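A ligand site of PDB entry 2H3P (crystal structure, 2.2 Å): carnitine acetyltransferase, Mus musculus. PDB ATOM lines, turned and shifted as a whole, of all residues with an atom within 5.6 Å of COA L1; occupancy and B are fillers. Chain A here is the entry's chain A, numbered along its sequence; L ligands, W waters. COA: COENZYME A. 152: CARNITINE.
Water W16 lies within hydrogen-bond range of an oxygen (O7A) of COA L1 (2.7 Å) and the side-chain amino group of Lys 397 (3.0 Å).
Water W14 lies within hydrogen-bond range of OAP of COA L1 (2.7 Å) and NH2 of Arg 478 (2.8 Å).
Water W3 lies within hydrogen-bond range of an oxygen (O4A) of COA L1 (2.8 Å) and the guanidinium group of Arg 478 (3.4 Å).
Water W10 lies within hydrogen-bond range of the side-chain amide nitrogen (NE2) of Gln 529 and an oxygen (O1A) of COA L1.
Water W2 lies within hydrogen-bond range of an oxygen (O5P) of COA L1 (3.0 Å) and the side-chain hydroxyl of Ser 430 (3.5 Å).
Water W1 lies within hydrogen-bond range of the side-chain hydroxyl (OG) of Ser 528 (2.9 Å), an oxygen (O3) of 152 L2 (3.0 Å) and a sulfur (S1P) of COA L1 (3.1 Å).
N6A of COA L1 sits close to N of Leu 401 (3.5 Å).
N of Pro 403 lies close to O1A of COA L1 (3.2 Å).
Merely in contact with COA L1: Ala 429 (3.4 Å), Ile 485 (3.4 Å), Pro 323 (3.4 Å), Glu 321 (3.5 Å), Ser 428 (3.5 Å), Thr 481 (3.6 Å), Val 530 (3.7 Å), Leu 137 (3.8 Å), Tyr 315 (3.96 Å) and Ser 528 (3.99 Å).
Hydrophobic or aromatic side chains that line COA L1: Leu 137, His 317, Pro 323, Pro 403, Ile 485 and Val 530.
The backbone NH (N) of Lys 393 lies within hydrogen-bond range of the backbone carbonyl oxygen (O) of Glu 556.
The backbone NH (N) of Gly 322 lies within hydrogen-bond range of the side-chain hydroxyl (OH) of Tyr 315.
The backbone NH (N) of Leu 401 sits at hydrogen-bond distance from the backbone carbonyl oxygen (O) of Pro 396.
OG of Ser 402 is in hydrogen-bond range of N of Ala 405 (3.4 Å).
The side-chain amino group (NZ) of Lys 397 is in salt-bridge range of the side-chain carboxylate (OE1) of Glu 556, at 3.3 Å.
OD1 of Asp 404 sits at hydrogen-bond distance from NE2 of Gln 529 (3.0 Å).
The backbone carbonyl oxygen of Ala 320 is in hydrogen-bond range of a ring nitrogen (ND1) of His 317 (3.0 Å).
The side-chain carboxylate of Asp 404 lies close to the side-chain carboxylate of Glu 427, at 2.5 Å.
S1P of COA L1 lies close to O3 of 152 L2, 2.8 Å away.
An oxygen (O1A) of COA L1 lies within hydrogen-bond range of the backbone NH (N) of Asp 404 (2.7 Å).
OG of Ser 402 is in hydrogen-bond range of O2A of COA L1, at 2.7 Å.
A nitrogen (N6A) of COA L1 is in hydrogen-bond range of the backbone carbonyl oxygen (O) of Lys 400 (3.2 Å).
NE2 of His 317 sits close to S1P of COA L1 (3.7 Å).
A nitrogen (N4P) of COA L1 is in hydrogen-bond range of the backbone carbonyl oxygen of Gln 529, 2.9 Å away.
The side-chain hydroxyl (OG) of Ser 428 sits at hydrogen-bond distance from an oxygen (O1B) of 152 L2, 2.6 Å away.
O9A of COA L1 is in salt-bridge range of NZ of Lys 397, 2.8 Å away.
The side-chain amino group (NZ) of Lys 393 is in salt-bridge range of an oxygen (O9A) of COA L1, at 3.0 Å.
N of Ser 430 sits at hydrogen-bond distance from O9P of COA L1, 2.8 Å away.
The guanidinium group (NH1) of Arg 478 lies within salt-bridge range of an oxygen (O4A) of COA L1 (2.7 Å).
OG1 of Thr 439 is in hydrogen-bond range of O1A of 152 L2, 2.8 Å away.
The backbone NH (N) of Gly 322 lies close to a sulfur (S1P) of COA L1, 3.3 Å away.
NE2 of His 317 is in hydrogen-bond range of O3 of 152 L2 (2.7 Å).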
ATOM      1  N   LEU A 137       9.278  -9.984  -6.101  1.00  0.00           N
ATOM      2  CA  LEU A 137       9.140 -10.822  -4.916  1.00  0.00           C
ATOM      3  C   LEU A 137       9.795 -12.180  -5.170  1.00  0.00           C
ATOM      4  O   LEU A 137      10.862 -12.468  -4.646  1.00  0.00           O
ATOM      5  CB  LEU A 137       7.661 -10.994  -4.548  1.00  0.00           C
ATOM      6  CG  LEU A 137       7.301 -11.656  -3.199  1.00  0.00           C
ATOM      7  CD1 LEU A 137       7.414 -13.157  -3.321  1.00  0.00           C
ATOM      8  CD2 LEU A 137       8.209 -11.128  -2.093  1.00  0.00           C
ATOM      9  N   TYR A 315      -3.972   2.328   9.279  1.00  0.00           N
ATOM     10  CA  TYR A 315      -4.571   2.424   7.957  1.00  0.00           C
ATOM     11  C   TYR A 315      -5.742   1.487   7.778  1.00  0.00           C
ATOM     12  O   TYR A 315      -5.801   0.416   8.381  1.00  0.00           O
ATOM     13  CB  TYR A 315      -3.518   2.143   6.884  1.00  0.00           C
ATOM     14  CG  TYR A 315      -3.181   0.684   6.697  1.00  0.00           C
ATOM     15  CD1 TYR A 315      -3.829  -0.088   5.737  1.00  0.00           C
ATOM     16  CD2 TYR A 315      -2.200   0.077   7.480  1.00  0.00           C
ATOM     17  CE1 TYR A 315      -3.506  -1.439   5.558  1.00  0.00           C
ATOM     18  CE2 TYR A 315      -1.861  -1.260   7.304  1.00  0.00           C
ATOM     19  CZ  TYR A 315      -2.516  -2.010   6.350  1.00  0.00           C
ATOM     20  OH  TYR A 315      -2.169  -3.341   6.175  1.00  0.00           O
ATOM     21  N   HIS A 317      -7.574  -1.252   6.222  1.00  0.00           N
ATOM     22  CA  HIS A 317      -7.150  -2.457   5.497  1.00  0.00           C
ATOM     23  C   HIS A 317      -7.788  -2.780   4.145  1.00  0.00           C
ATOM     24  O   HIS A 317      -7.239  -3.564   3.383  1.00  0.00           O
ATOM     25  CB  HIS A 317      -7.314  -3.674   6.405  1.00  0.00           C
ATOM     26  CG  HIS A 317      -6.216  -4.688   6.264  1.00  0.00           C
ATOM     27  ND1 HIS A 317      -5.553  -4.904   5.068  1.00  0.00           N
ATOM     28  CD2 HIS A 317      -5.687  -5.568   7.142  1.00  0.00           C
ATOM     29  CE1 HIS A 317      -4.668  -5.870   5.231  1.00  0.00           C
ATOM     30  NE2 HIS A 317      -4.722  -6.287   6.481  1.00  0.00           N
ATOM     31  N   ALA A 320      -5.292  -1.766   1.078  1.00  0.00           N
ATOM     32  CA  ALA A 320      -4.097  -2.537   0.763  1.00  0.00           C
ATOM     33  C   ALA A 320      -3.523  -3.344   1.905  1.00  0.00           C
ATOM     34  O   ALA A 320      -4.082  -3.379   3.006  1.00  0.00           O
ATOM     35  CB  ALA A 320      -3.027  -1.594   0.240  1.00  0.00           C
ATOM     36  N   GLU A 321      -2.409  -4.024   1.633  1.00  0.00           N
ATOM     37  CA  GLU A 321      -1.723  -4.802   2.646  1.00  0.00           C
ATOM     38  C   GLU A 321      -0.583  -3.973   3.218  1.00  0.00           C
ATOM     39  O   GLU A 321      -0.440  -2.786   2.905  1.00  0.00           O
ATOM     40  CB  GLU A 321      -1.161  -6.103   2.063  1.00  0.00           C
ATOM     41  CG  GLU A 321      -2.038  -7.316   2.352  1.00  0.00           C
ATOM     42  CD  GLU A 321      -3.379  -7.209   1.677  1.00  0.00           C
ATOM     43  OE1 GLU A 321      -3.415  -7.315   0.437  1.00  0.00           O
ATOM     44  OE2 GLU A 321      -4.382  -7.004   2.383  1.00  0.00           O
ATOM     45  N   GLY A 322       0.233  -4.611   4.058  1.00  0.00           N
ATOM     46  CA  GLY A 322       1.336  -3.908   4.700  1.00  0.00           C
ATOM     47  C   GLY A 322       2.496  -3.455   3.825  1.00  0.00           C
ATOM     48  O   GLY A 322       2.937  -2.305   3.945  1.00  0.00           O
ATOM     49  N   PRO A 323       3.034  -4.329   2.944  1.00  0.00           N
ATOM     50  CA  PRO A 323       4.155  -3.943   2.091  1.00  0.00           C
ATOM     51  C   PRO A 323       4.025  -2.556   1.431  1.00  0.00           C
ATOM     52  O   PRO A 323       4.919  -1.720   1.575  1.00  0.00           O
ATOM     53  CB  PRO A 323       4.233  -5.093   1.091  1.00  0.00           C
ATOM     54  CG  PRO A 323       3.868  -6.267   1.969  1.00  0.00           C
ATOM     55  CD  PRO A 323       2.677  -5.736   2.734  1.00  0.00           C
ATOM     56  N   LYS A 393      17.532 -11.693  10.924  1.00  0.00           N
ATOM     57  CA  LYS A 393      17.630 -12.573   9.757  1.00  0.00           C
ATOM     58  C   LYS A 393      19.038 -13.129   9.637  1.00  0.00           C
ATOM     59  O   LYS A 393      19.251 -14.154   8.978  1.00  0.00           O
ATOM     60  CB  LYS A 393      17.297 -11.797   8.486  1.00  0.00           C
ATOM     61  CG  LYS A 393      15.929 -11.161   8.499  1.00  0.00           C
ATOM     62  CD  LYS A 393      15.670 -10.465   7.170  1.00  0.00           C
ATOM     63  CE  LYS A 393      16.555  -9.237   7.011  1.00  0.00           C
ATOM     64  NZ  LYS A 393      16.267  -8.544   5.721  1.00  0.00           N
ATOM     65  N   PRO A 396      19.521 -17.067  10.957  1.00  0.00           N
ATOM     66  CA  PRO A 396      18.875 -18.043  10.069  1.00  0.00           C
ATOM     67  C   PRO A 396      19.621 -18.163   8.744  1.00  0.00           C
ATOM     68  O   PRO A 396      19.837 -19.266   8.239  1.00  0.00           O
ATOM     69  CB  PRO A 396      17.465 -17.464   9.883  1.00  0.00           C
ATOM     70  CG  PRO A 396      17.229 -16.772  11.179  1.00  0.00           C
ATOM     71  CD  PRO A 396      18.548 -16.074  11.440  1.00  0.00           C
ATOM     72  N   LYS A 397      20.031 -17.021   8.198  1.00  0.00           N
ATOM     73  CA  LYS A 397      20.744 -17.017   6.929  1.00  0.00           C
ATOM     74  C   LYS A 397      22.105 -17.697   7.035  1.00  0.00           C
ATOM     75  O   LYS A 397      22.496 -18.438   6.127  1.00  0.00           O
ATOM     76  CB  LYS A 397      20.886 -15.589   6.409  1.00  0.00           C
ATOM     77  CG  LYS A 397      19.533 -15.007   5.995  1.00  0.00           C
ATOM     78  CD  LYS A 397      19.633 -13.795   5.101  1.00  0.00           C
ATOM     79  CE  LYS A 397      20.087 -12.582   5.859  1.00  0.00           C
ATOM     80  NZ  LYS A 397      20.076 -11.378   4.973  1.00  0.00           N
ATOM     81  N   LYS A 400      21.716 -21.162   6.470  1.00  0.00           N
ATOM     82  CA  LYS A 400      21.132 -21.529   5.180  1.00  0.00           C
ATOM     83  C   LYS A 400      19.675 -21.876   5.404  1.00  0.00           C
ATOM     84  O   LYS A 400      19.188 -22.888   4.897  1.00  0.00           O
ATOM     85  CB  LYS A 400      21.860 -22.724   4.555  1.00  0.00           C
ATOM     86  CG  LYS A 400      23.315 -22.454   4.151  1.00  0.00           C
ATOM     87  CD  LYS A 400      23.415 -21.253   3.235  1.00  0.00           C
ATOM     88  CE  LYS A 400      24.862 -20.854   2.962  1.00  0.00           C
ATOM     89  NZ  LYS A 400      24.954 -19.586   2.168  1.00  0.00           N
ATOM     90  N   LEU A 401      18.978 -21.041   6.157  1.00  0.00           N
ATOM     91  CA  LEU A 401      17.569 -21.281   6.439  1.00  0.00           C
ATOM     92  C   LEU A 401      16.782 -19.999   6.226  1.00  0.00           C
ATOM     93  O   LEU A 401      17.286 -18.906   6.502  1.00  0.00           O
ATOM     94  CB  LEU A 401      17.377 -21.752   7.878  1.00  0.00           C
ATOM     95  CG  LEU A 401      18.014 -23.078   8.293  1.00  0.00           C
ATOM     96  CD1 LEU A 401      17.803 -23.268   9.794  1.00  0.00           C
ATOM     97  CD2 LEU A 401      17.384 -24.235   7.530  1.00  0.00           C
ATOM     98  N   SER A 402      15.556 -20.124   5.736  1.00  0.00           N
ATOM     99  CA  SER A 402      14.721 -18.955   5.513  1.00  0.00           C
ATOM    100  C   SER A 402      14.346 -18.338   6.847  1.00  0.00           C
ATOM    101  O   SER A 402      13.771 -19.007   7.715  1.00  0.00           O
ATOM    102  CB  SER A 402      13.436 -19.346   4.780  1.00  0.00           C
ATOM    103  OG  SER A 402      12.476 -18.304   4.889  1.00  0.00           O
ATOM    104  N   PRO A 403      14.667 -17.043   7.043  1.00  0.00           N
ATOM    105  CA  PRO A 403      14.351 -16.338   8.279  1.00  0.00           C
ATOM    106  C   PRO A 403      12.877 -16.406   8.644  1.00  0.00           C
ATOM    107  O   PRO A 403      12.525 -16.698   9.798  1.00  0.00           O
ATOM    108  CB  PRO A 403      14.788 -14.909   7.980  1.00  0.00           C
ATOM    109  CG  PRO A 403      15.978 -15.120   7.096  1.00  0.00           C
ATOM    110  CD  PRO A 403      15.512 -16.209   6.155  1.00  0.00           C
ATOM    111  N   ASP A 404      12.014 -16.146   7.674  1.00  0.00           N
ATOM    112  CA  ASP A 404      10.583 -16.185   7.945  1.00  0.00           C
ATOM    113  C   ASP A 404      10.143 -17.571   8.374  1.00  0.00           C
ATOM    114  O   ASP A 404       9.383 -17.717   9.327  1.00  0.00           O
ATOM    115  CB  ASP A 404       9.782 -15.754   6.723  1.00  0.00           C
ATOM    116  CG  ASP A 404       8.309 -15.594   7.045  1.00  0.00           C
ATOM    117  OD1 ASP A 404       7.977 -14.703   7.850  1.00  0.00           O
ATOM    118  OD2 ASP A 404       7.489 -16.370   6.491  1.00  0.00           O
ATOM    119  N   ALA A 405      10.617 -18.604   7.674  1.00  0.00           N
ATOM    120  CA  ALA A 405      10.259 -19.964   8.027  1.00  0.00           C
ATOM    121  C   ALA A 405      10.837 -20.312   9.396  1.00  0.00           C
ATOM    122  O   ALA A 405      10.215 -21.035  10.178  1.00  0.00           O
ATOM    123  CB  ALA A 405      10.748 -20.937   6.960  1.00  0.00           C
ATOM    124  N   GLU A 427      -0.695 -17.255   7.963  1.00  0.00           N
ATOM    125  CA  GLU A 427       0.387 -16.310   7.705  1.00  0.00           C
ATOM    126  C   GLU A 427       0.097 -15.680   6.342  1.00  0.00           C
ATOM    127  O   GLU A 427      -0.078 -16.387   5.347  1.00  0.00           O
ATOM    128  CB  GLU A 427       1.782 -16.973   7.658  1.00  0.00           C
ATOM    129  CG  GLU A 427       2.825 -15.980   7.119  1.00  0.00           C
ATOM    130  CD  GLU A 427       4.258 -16.483   7.067  1.00  0.00           C
ATOM    131  OE1 GLU A 427       4.470 -17.705   7.015  1.00  0.00           O
ATOM    132  OE2 GLU A 427       5.186 -15.648   7.059  1.00  0.00           O
ATOM    133  N   SER A 428       0.048 -14.357   6.310  1.00  0.00           N
ATOM    134  CA  SER A 428      -0.213 -13.612   5.075  1.00  0.00           C
ATOM    135  C   SER A 428       0.802 -13.890   3.969  1.00  0.00           C
ATOM    136  O   SER A 428       2.010 -13.807   4.192  1.00  0.00           O
ATOM    137  CB  SER A 428      -0.214 -12.100   5.353  1.00  0.00           C
ATOM    138  OG  SER A 428      -1.280 -11.717   6.199  1.00  0.00           O
ATOM    139  N   ALA A 429       0.310 -14.211   2.776  1.00  0.00           N
ATOM    140  CA  ALA A 429       1.181 -14.435   1.633  1.00  0.00           C
ATOM    141  C   ALA A 429       0.733 -13.458   0.547  1.00  0.00           C
ATOM    142  O   ALA A 429      -0.451 -13.369   0.253  1.00  0.00           O
ATOM    143  CB  ALA A 429       1.075 -15.876   1.138  1.00  0.00           C
ATOM    144  N   SER A 430       1.689 -12.731  -0.032  1.00  0.00           N
ATOM    145  CA  SER A 430       1.378 -11.756  -1.067  1.00  0.00           C
ATOM    146  C   SER A 430       1.166 -12.435  -2.415  1.00  0.00           C
ATOM    147  O   SER A 430       1.951 -13.294  -2.824  1.00  0.00           O
ATOM    148  CB  SER A 430       2.513 -10.740  -1.189  1.00  0.00           C
ATOM    149  OG  SER A 430       2.271  -9.840  -2.260  1.00  0.00           O
ATOM    150  N   THR A 439      -3.801 -11.289  -1.317  1.00  0.00           N
ATOM    151  CA  THR A 439      -3.166 -12.305  -0.487  1.00  0.00           C
ATOM    152  C   THR A 439      -3.742 -13.702  -0.595  1.00  0.00           C
ATOM    153  O   THR A 439      -4.833 -13.920  -1.129  1.00  0.00           O
ATOM    154  CB  THR A 439      -3.268 -11.965   1.013  1.00  0.00           C
ATOM    155  OG1 THR A 439      -4.615 -12.152   1.454  1.00  0.00           O
ATOM    156  CG2 THR A 439      -2.846 -10.548   1.253  1.00  0.00           C
ATOM    157  N   ILE A 442      -0.842 -19.036   3.942  1.00  0.00           N
ATOM    158  CA  ILE A 442       0.240 -19.971   4.193  1.00  0.00           C
ATOM    159  C   ILE A 442      -0.101 -20.580   5.545  1.00  0.00           C
ATOM    160  O   ILE A 442      -0.365 -19.860   6.510  1.00  0.00           O
ATOM    161  CB  ILE A 442       1.595 -19.256   4.273  1.00  0.00           C
ATOM    162  CG1 ILE A 442       1.943 -18.698   2.892  1.00  0.00           C
ATOM    163  CG2 ILE A 442       2.658 -20.209   4.764  1.00  0.00           C
ATOM    164  CD1 ILE A 442       3.266 -17.954   2.848  1.00  0.00           C
ATOM    165  N   GLN A 475      12.096 -26.052   5.749  1.00  0.00           N
ATOM    166  CA  GLN A 475      12.017 -26.244   4.303  1.00  0.00           C
ATOM    167  C   GLN A 475      10.580 -26.467   3.842  1.00  0.00           C
ATOM    168  O   GLN A 475      10.181 -25.978   2.775  1.00  0.00           O
ATOM    169  CB  GLN A 475      12.911 -27.401   3.856  1.00  0.00           C
ATOM    170  CG  GLN A 475      14.400 -27.074   3.884  1.00  0.00           C
ATOM    171  CD  GLN A 475      14.740 -25.833   3.069  1.00  0.00           C
ATOM    172  OE1 GLN A 475      14.450 -25.751   1.869  1.00  0.00           O
ATOM    173  NE2 GLN A 475      15.360 -24.849   3.719  1.00  0.00           N
ATOM    174  N   ARG A 478       8.975 -23.180   3.645  1.00  0.00           N
ATOM    175  CA  ARG A 478       9.483 -22.373   2.525  1.00  0.00           C
ATOM    176  C   ARG A 478       8.838 -22.871   1.230  1.00  0.00           C
ATOM    177  O   ARG A 478       8.554 -22.077   0.329  1.00  0.00           O
ATOM    178  CB  ARG A 478      11.010 -22.509   2.424  1.00  0.00           C
ATOM    179  CG  ARG A 478      11.637 -21.783   1.222  1.00  0.00           C
ATOM    180  CD  ARG A 478      11.515 -20.254   1.329  1.00  0.00           C
ATOM    181  NE  ARG A 478      10.620 -19.683   0.328  1.00  0.00           N
ATOM    182  CZ  ARG A 478      10.356 -18.387   0.220  1.00  0.00           C
ATOM    183  NH1 ARG A 478      10.934 -17.525   1.053  1.00  0.00           N
ATOM    184  NH2 ARG A 478       9.521 -17.946  -0.721  1.00  0.00           N
ATOM    185  N   THR A 481       5.413 -21.579   1.112  1.00  0.00           N
ATOM    186  CA  THR A 481       5.494 -20.159   0.805  1.00  0.00           C
ATOM    187  C   THR A 481       5.670 -19.925  -0.699  1.00  0.00           C
ATOM    188  O   THR A 481       5.027 -19.054  -1.270  1.00  0.00           O
ATOM    189  CB  THR A 481       6.672 -19.487   1.562  1.00  0.00           C
ATOM    190  OG1 THR A 481       6.495 -19.656   2.968  1.00  0.00           O
ATOM    191  CG2 THR A 481       6.728 -18.006   1.247  1.00  0.00           C
ATOM    192  N   ILE A 485       2.819 -17.695  -2.981  1.00  0.00           N
ATOM    193  CA  ILE A 485       3.073 -16.485  -3.750  1.00  0.00           C
ATOM    194  C   ILE A 485       2.832 -16.712  -5.238  1.00  0.00           C
ATOM    195  O   ILE A 485       2.572 -15.768  -5.983  1.00  0.00           O
ATOM    196  CB  ILE A 485       4.521 -15.986  -3.515  1.00  0.00           C
ATOM    197  CG1 ILE A 485       5.518 -17.109  -3.771  1.00  0.00           C
ATOM    198  CG2 ILE A 485       4.646 -15.465  -2.096  1.00  0.00           C
ATOM    199  CD1 ILE A 485       6.963 -16.703  -3.524  1.00  0.00           C
ATOM    200  N   SER A 528       1.550 -12.414  10.246  1.00  0.00           N
ATOM    201  CA  SER A 528       2.020 -11.809   9.016  1.00  0.00           C
ATOM    202  C   SER A 528       3.386 -11.194   9.244  1.00  0.00           C
ATOM    203  O   SER A 528       3.777 -10.914  10.374  1.00  0.00           O
ATOM    204  CB  SER A 528       1.067 -10.720   8.521  1.00  0.00           C
ATOM    205  OG  SER A 528       1.219  -9.536   9.270  1.00  0.00           O
ATOM    206  N   GLN A 529       4.104 -10.991   8.153  1.00  0.00           N
ATOM    207  CA  GLN A 529       5.408 -10.383   8.217  1.00  0.00           C
ATOM    208  C   GLN A 529       5.331  -9.110   7.390  1.00  0.00           C
ATOM    209  O   GLN A 529       4.753  -9.110   6.296  1.00  0.00           O
ATOM    210  CB  GLN A 529       6.445 -11.323   7.608  1.00  0.00           C
ATOM    211  CG  GLN A 529       7.854 -10.914   7.915  1.00  0.00           C
ATOM    212  CD  GLN A 529       8.835 -11.311   6.830  1.00  0.00           C
ATOM    213  OE1 GLN A 529       8.858 -10.715   5.759  1.00  0.00           O
ATOM    214  NE2 GLN A 529       9.666 -12.313   7.113  1.00  0.00           N
ATOM    215  N   VAL A 530       5.872  -8.025   7.912  1.00  0.00           N
ATOM    216  CA  VAL A 530       5.859  -6.778   7.155  1.00  0.00           C
ATOM    217  C   VAL A 530       7.273  -6.184   7.168  1.00  0.00           C
ATOM    218  O   VAL A 530       7.588  -5.336   7.999  1.00  0.00           O
ATOM    219  CB  VAL A 530       4.857  -5.754   7.757  1.00  0.00           C
ATOM    220  CG1 VAL A 530       4.835  -4.494   6.892  1.00  0.00           C
ATOM    221  CG2 VAL A 530       3.450  -6.355   7.830  1.00  0.00           C
ATOM    222  N   PRO A 531       8.131  -6.633   6.238  1.00  0.00           N
ATOM    223  CA  PRO A 531       9.510  -6.149   6.130  1.00  0.00           C
ATOM    224  C   PRO A 531       9.563  -4.635   5.923  1.00  0.00           C
ATOM    225  O   PRO A 531       8.620  -4.054   5.386  1.00  0.00           O
ATOM    226  CB  PRO A 531      10.043  -6.878   4.890  1.00  0.00           C
ATOM    227  CG  PRO A 531       9.209  -8.092   4.793  1.00  0.00           C
ATOM    228  CD  PRO A 531       7.823  -7.609   5.184  1.00  0.00           C
ATOM    229  N   GLU A 556      17.902  -7.307  10.188  1.00  0.00           N
ATOM    230  CA  GLU A 556      19.148  -8.068  10.100  1.00  0.00           C
ATOM    231  C   GLU A 556      19.662  -8.570  11.450  1.00  0.00           C
ATOM    232  O   GLU A 556      19.941  -9.750  11.599  1.00  0.00           O
ATOM    233  CB  GLU A 556      20.217  -7.220   9.396  1.00  0.00           C
ATOM    234  CG  GLU A 556      21.523  -7.936   9.095  1.00  0.00           C
ATOM    235  CD  GLU A 556      21.353  -9.130   8.158  1.00  0.00           C
ATOM    236  OE1 GLU A 556      20.436  -9.108   7.302  1.00  0.00           O
ATOM    237  OE2 GLU A 556      22.153 -10.096   8.268  1.00  0.00           O
HETATM  238  N1A COA L   1      19.762 -19.189   3.061  1.00  0.00           N
HETATM  239  C2A COA L   1      20.229 -17.939   3.138  1.00  0.00           C
HETATM  240  N3A COA L   1      19.412 -16.898   2.985  1.00  0.00           N
HETATM  241  C4A COA L   1      18.072 -17.077   2.793  1.00  0.00           C
HETATM  242  C5A COA L   1      17.571 -18.365   2.704  1.00  0.00           C
HETATM  243  C6A COA L   1      18.446 -19.431   2.877  1.00  0.00           C
HETATM  244  N6A COA L   1      17.990 -20.687   2.845  1.00  0.00           N
HETATM  245  N7A COA L   1      16.263 -18.270   2.517  1.00  0.00           N
HETATM  246  C8A COA L   1      15.948 -16.967   2.453  1.00  0.00           C
HETATM  247  N9A COA L   1      17.062 -16.242   2.619  1.00  0.00           N
HETATM  248  C1B COA L   1      17.157 -14.748   2.687  1.00  0.00           C
HETATM  249  C2B COA L   1      16.380 -14.050   1.589  1.00  0.00           C
HETATM  250  O2B COA L   1      17.204 -14.005   0.406  1.00  0.00           O
HETATM  251  C3B COA L   1      16.214 -12.672   2.157  1.00  0.00           C
HETATM  252  O3B COA L   1      17.456 -11.973   2.025  1.00  0.00           O
HETATM  253  P3B COA L   1      17.541 -10.397   2.336  1.00  0.00           P
HETATM  254  O7A COA L   1      18.886  -9.950   1.582  1.00  0.00           O
HETATM  255  O8A COA L   1      16.366  -9.756   1.703  1.00  0.00           O
HETATM  256  O9A COA L   1      17.753 -10.224   3.798  1.00  0.00           O
HETATM  257  C4B COA L   1      15.931 -12.931   3.641  1.00  0.00           C
HETATM  258  O4B COA L   1      16.602 -14.212   3.926  1.00  0.00           O
HETATM  259  C5B COA L   1      14.429 -13.092   3.922  1.00  0.00           C
HETATM  260  O5B COA L   1      13.878 -14.191   3.177  1.00  0.00           O
HETATM  261  P1A COA L   1      12.674 -15.054   3.815  1.00  0.00           P
HETATM  262  O1A COA L   1      12.860 -15.103   5.282  1.00  0.00           O
HETATM  263  O2A COA L   1      12.543 -16.329   3.080  1.00  0.00           O
HETATM  264  O3A COA L   1      11.377 -14.122   3.532  1.00  0.00           O
HETATM  265  P2A COA L   1      10.929 -13.704   2.030  1.00  0.00           P
HETATM  266  O4A COA L   1      11.027 -14.861   1.111  1.00  0.00           O
HETATM  267  O5A COA L   1      11.611 -12.446   1.655  1.00  0.00           O
HETATM  268  O6A COA L   1       9.387 -13.380   2.242  1.00  0.00           O
HETATM  269  CBP COA L   1       7.051 -13.850   2.657  1.00  0.00           C
HETATM  270  CCP COA L   1       8.454 -14.430   2.522  1.00  0.00           C
HETATM  271  CDP COA L   1       7.052 -12.801   3.784  1.00  0.00           C
HETATM  272  CEP COA L   1       6.059 -14.970   3.021  1.00  0.00           C
HETATM  273  CAP COA L   1       6.661 -13.182   1.305  1.00  0.00           C
HETATM  274  OAP COA L   1       6.727 -14.153   0.260  1.00  0.00           O
HETATM  275  C9P COA L   1       5.265 -12.566   1.357  1.00  0.00           C
HETATM  276  O9P COA L   1       4.274 -13.202   1.008  1.00  0.00           O
HETATM  277  N8P COA L   1       5.246 -11.314   1.811  1.00  0.00           N
HETATM  278  C7P COA L   1       4.010 -10.542   1.943  1.00  0.00           C
HETATM  279  C6P COA L   1       3.414 -10.678   3.350  1.00  0.00           C
HETATM  280  C5P COA L   1       2.319  -9.648   3.556  1.00  0.00           C
HETATM  281  O5P COA L   1       1.453  -9.466   2.690  1.00  0.00           O
HETATM  282  N4P COA L   1       2.387  -8.982   4.709  1.00  0.00           N
HETATM  283  C3P COA L   1       1.439  -7.909   5.104  1.00  0.00           C
HETATM  284  C2P COA L   1       0.036  -8.474   5.393  1.00  0.00           C
HETATM  285  S1P COA L   1      -1.170  -7.142   5.722  1.00  0.00           S
HETATM  286  C1  152 L   2      -4.366 -10.697   4.731  1.00  0.00           C
HETATM  287  O1A 152 L   2      -5.259 -10.794   3.853  1.00  0.00           O
HETATM  288  O1B 152 L   2      -3.572 -11.637   5.011  1.00  0.00           O
HETATM  289  C2  152 L   2      -4.236  -9.392   5.488  1.00  0.00           C
HETATM  290  C3  152 L   2      -3.717  -9.583   6.912  1.00  0.00           C
HETATM  291  O3  152 L   2      -3.139  -8.337   7.336  1.00  0.00           O
HETATM  292  C4  152 L   2      -4.916  -9.918   7.829  1.00  0.00           C
HETATM  293  N5  152 L   2      -4.462 -10.465   9.121  1.00  0.00           N
HETATM  294  C5A 152 L   2      -3.403 -11.451   8.912  1.00  0.00           C
HETATM  295  C5B 152 L   2      -3.957  -9.377   9.974  1.00  0.00           C
HETATM  296  C5C 152 L   2      -5.591 -11.108   9.781  1.00  0.00           C
HETATM  297  O   HOH W   1      -0.669  -7.336   8.775  1.00  0.00           O
HETATM  298  O   HOH W   2       1.271  -7.708   0.311  1.00  0.00           O
HETATM  299  O   HOH W   3      13.476 -15.531  -0.057  1.00  0.00           O
HETATM  300  O   HOH W   4      19.987  -8.275   3.184  1.00  0.00           O
HETATM  301  O   HOH W   5      16.493 -10.277  -1.396  1.00  0.00           O
HETATM  302  O   HOH W   6      15.264 -20.718   1.774  1.00  0.00           O
HETATM  303  O   HOH W   7       7.423  -9.912   2.592  1.00  0.00           O
HETATM  304  O   HOH W   8      21.070 -14.821   2.186  1.00  0.00           O
HETATM  305  O   HOH W   9      17.491  -7.391   2.145  1.00  0.00           O
HETATM  306  O   HOH W  10      12.235 -12.694   6.729  1.00  0.00           O
HETATM  307  O   HOH W  11       3.807 -12.716   6.060  1.00  0.00           O
HETATM  308  O   HOH W  12      17.482 -17.054  -1.023  1.00  0.00           O
HETATM  309  O   HOH W  13      19.583 -12.803  -0.540  1.00  0.00           O
HETATM  310  O   HOH W  14       8.935 -15.242  -0.906  1.00  0.00           O
HETATM  311  O   HOH W  15      10.479 -10.307   2.173  1.00  0.00           O
HETATM  312  O   HOH W  16      21.026 -11.464   2.098  1.00  0.00           O
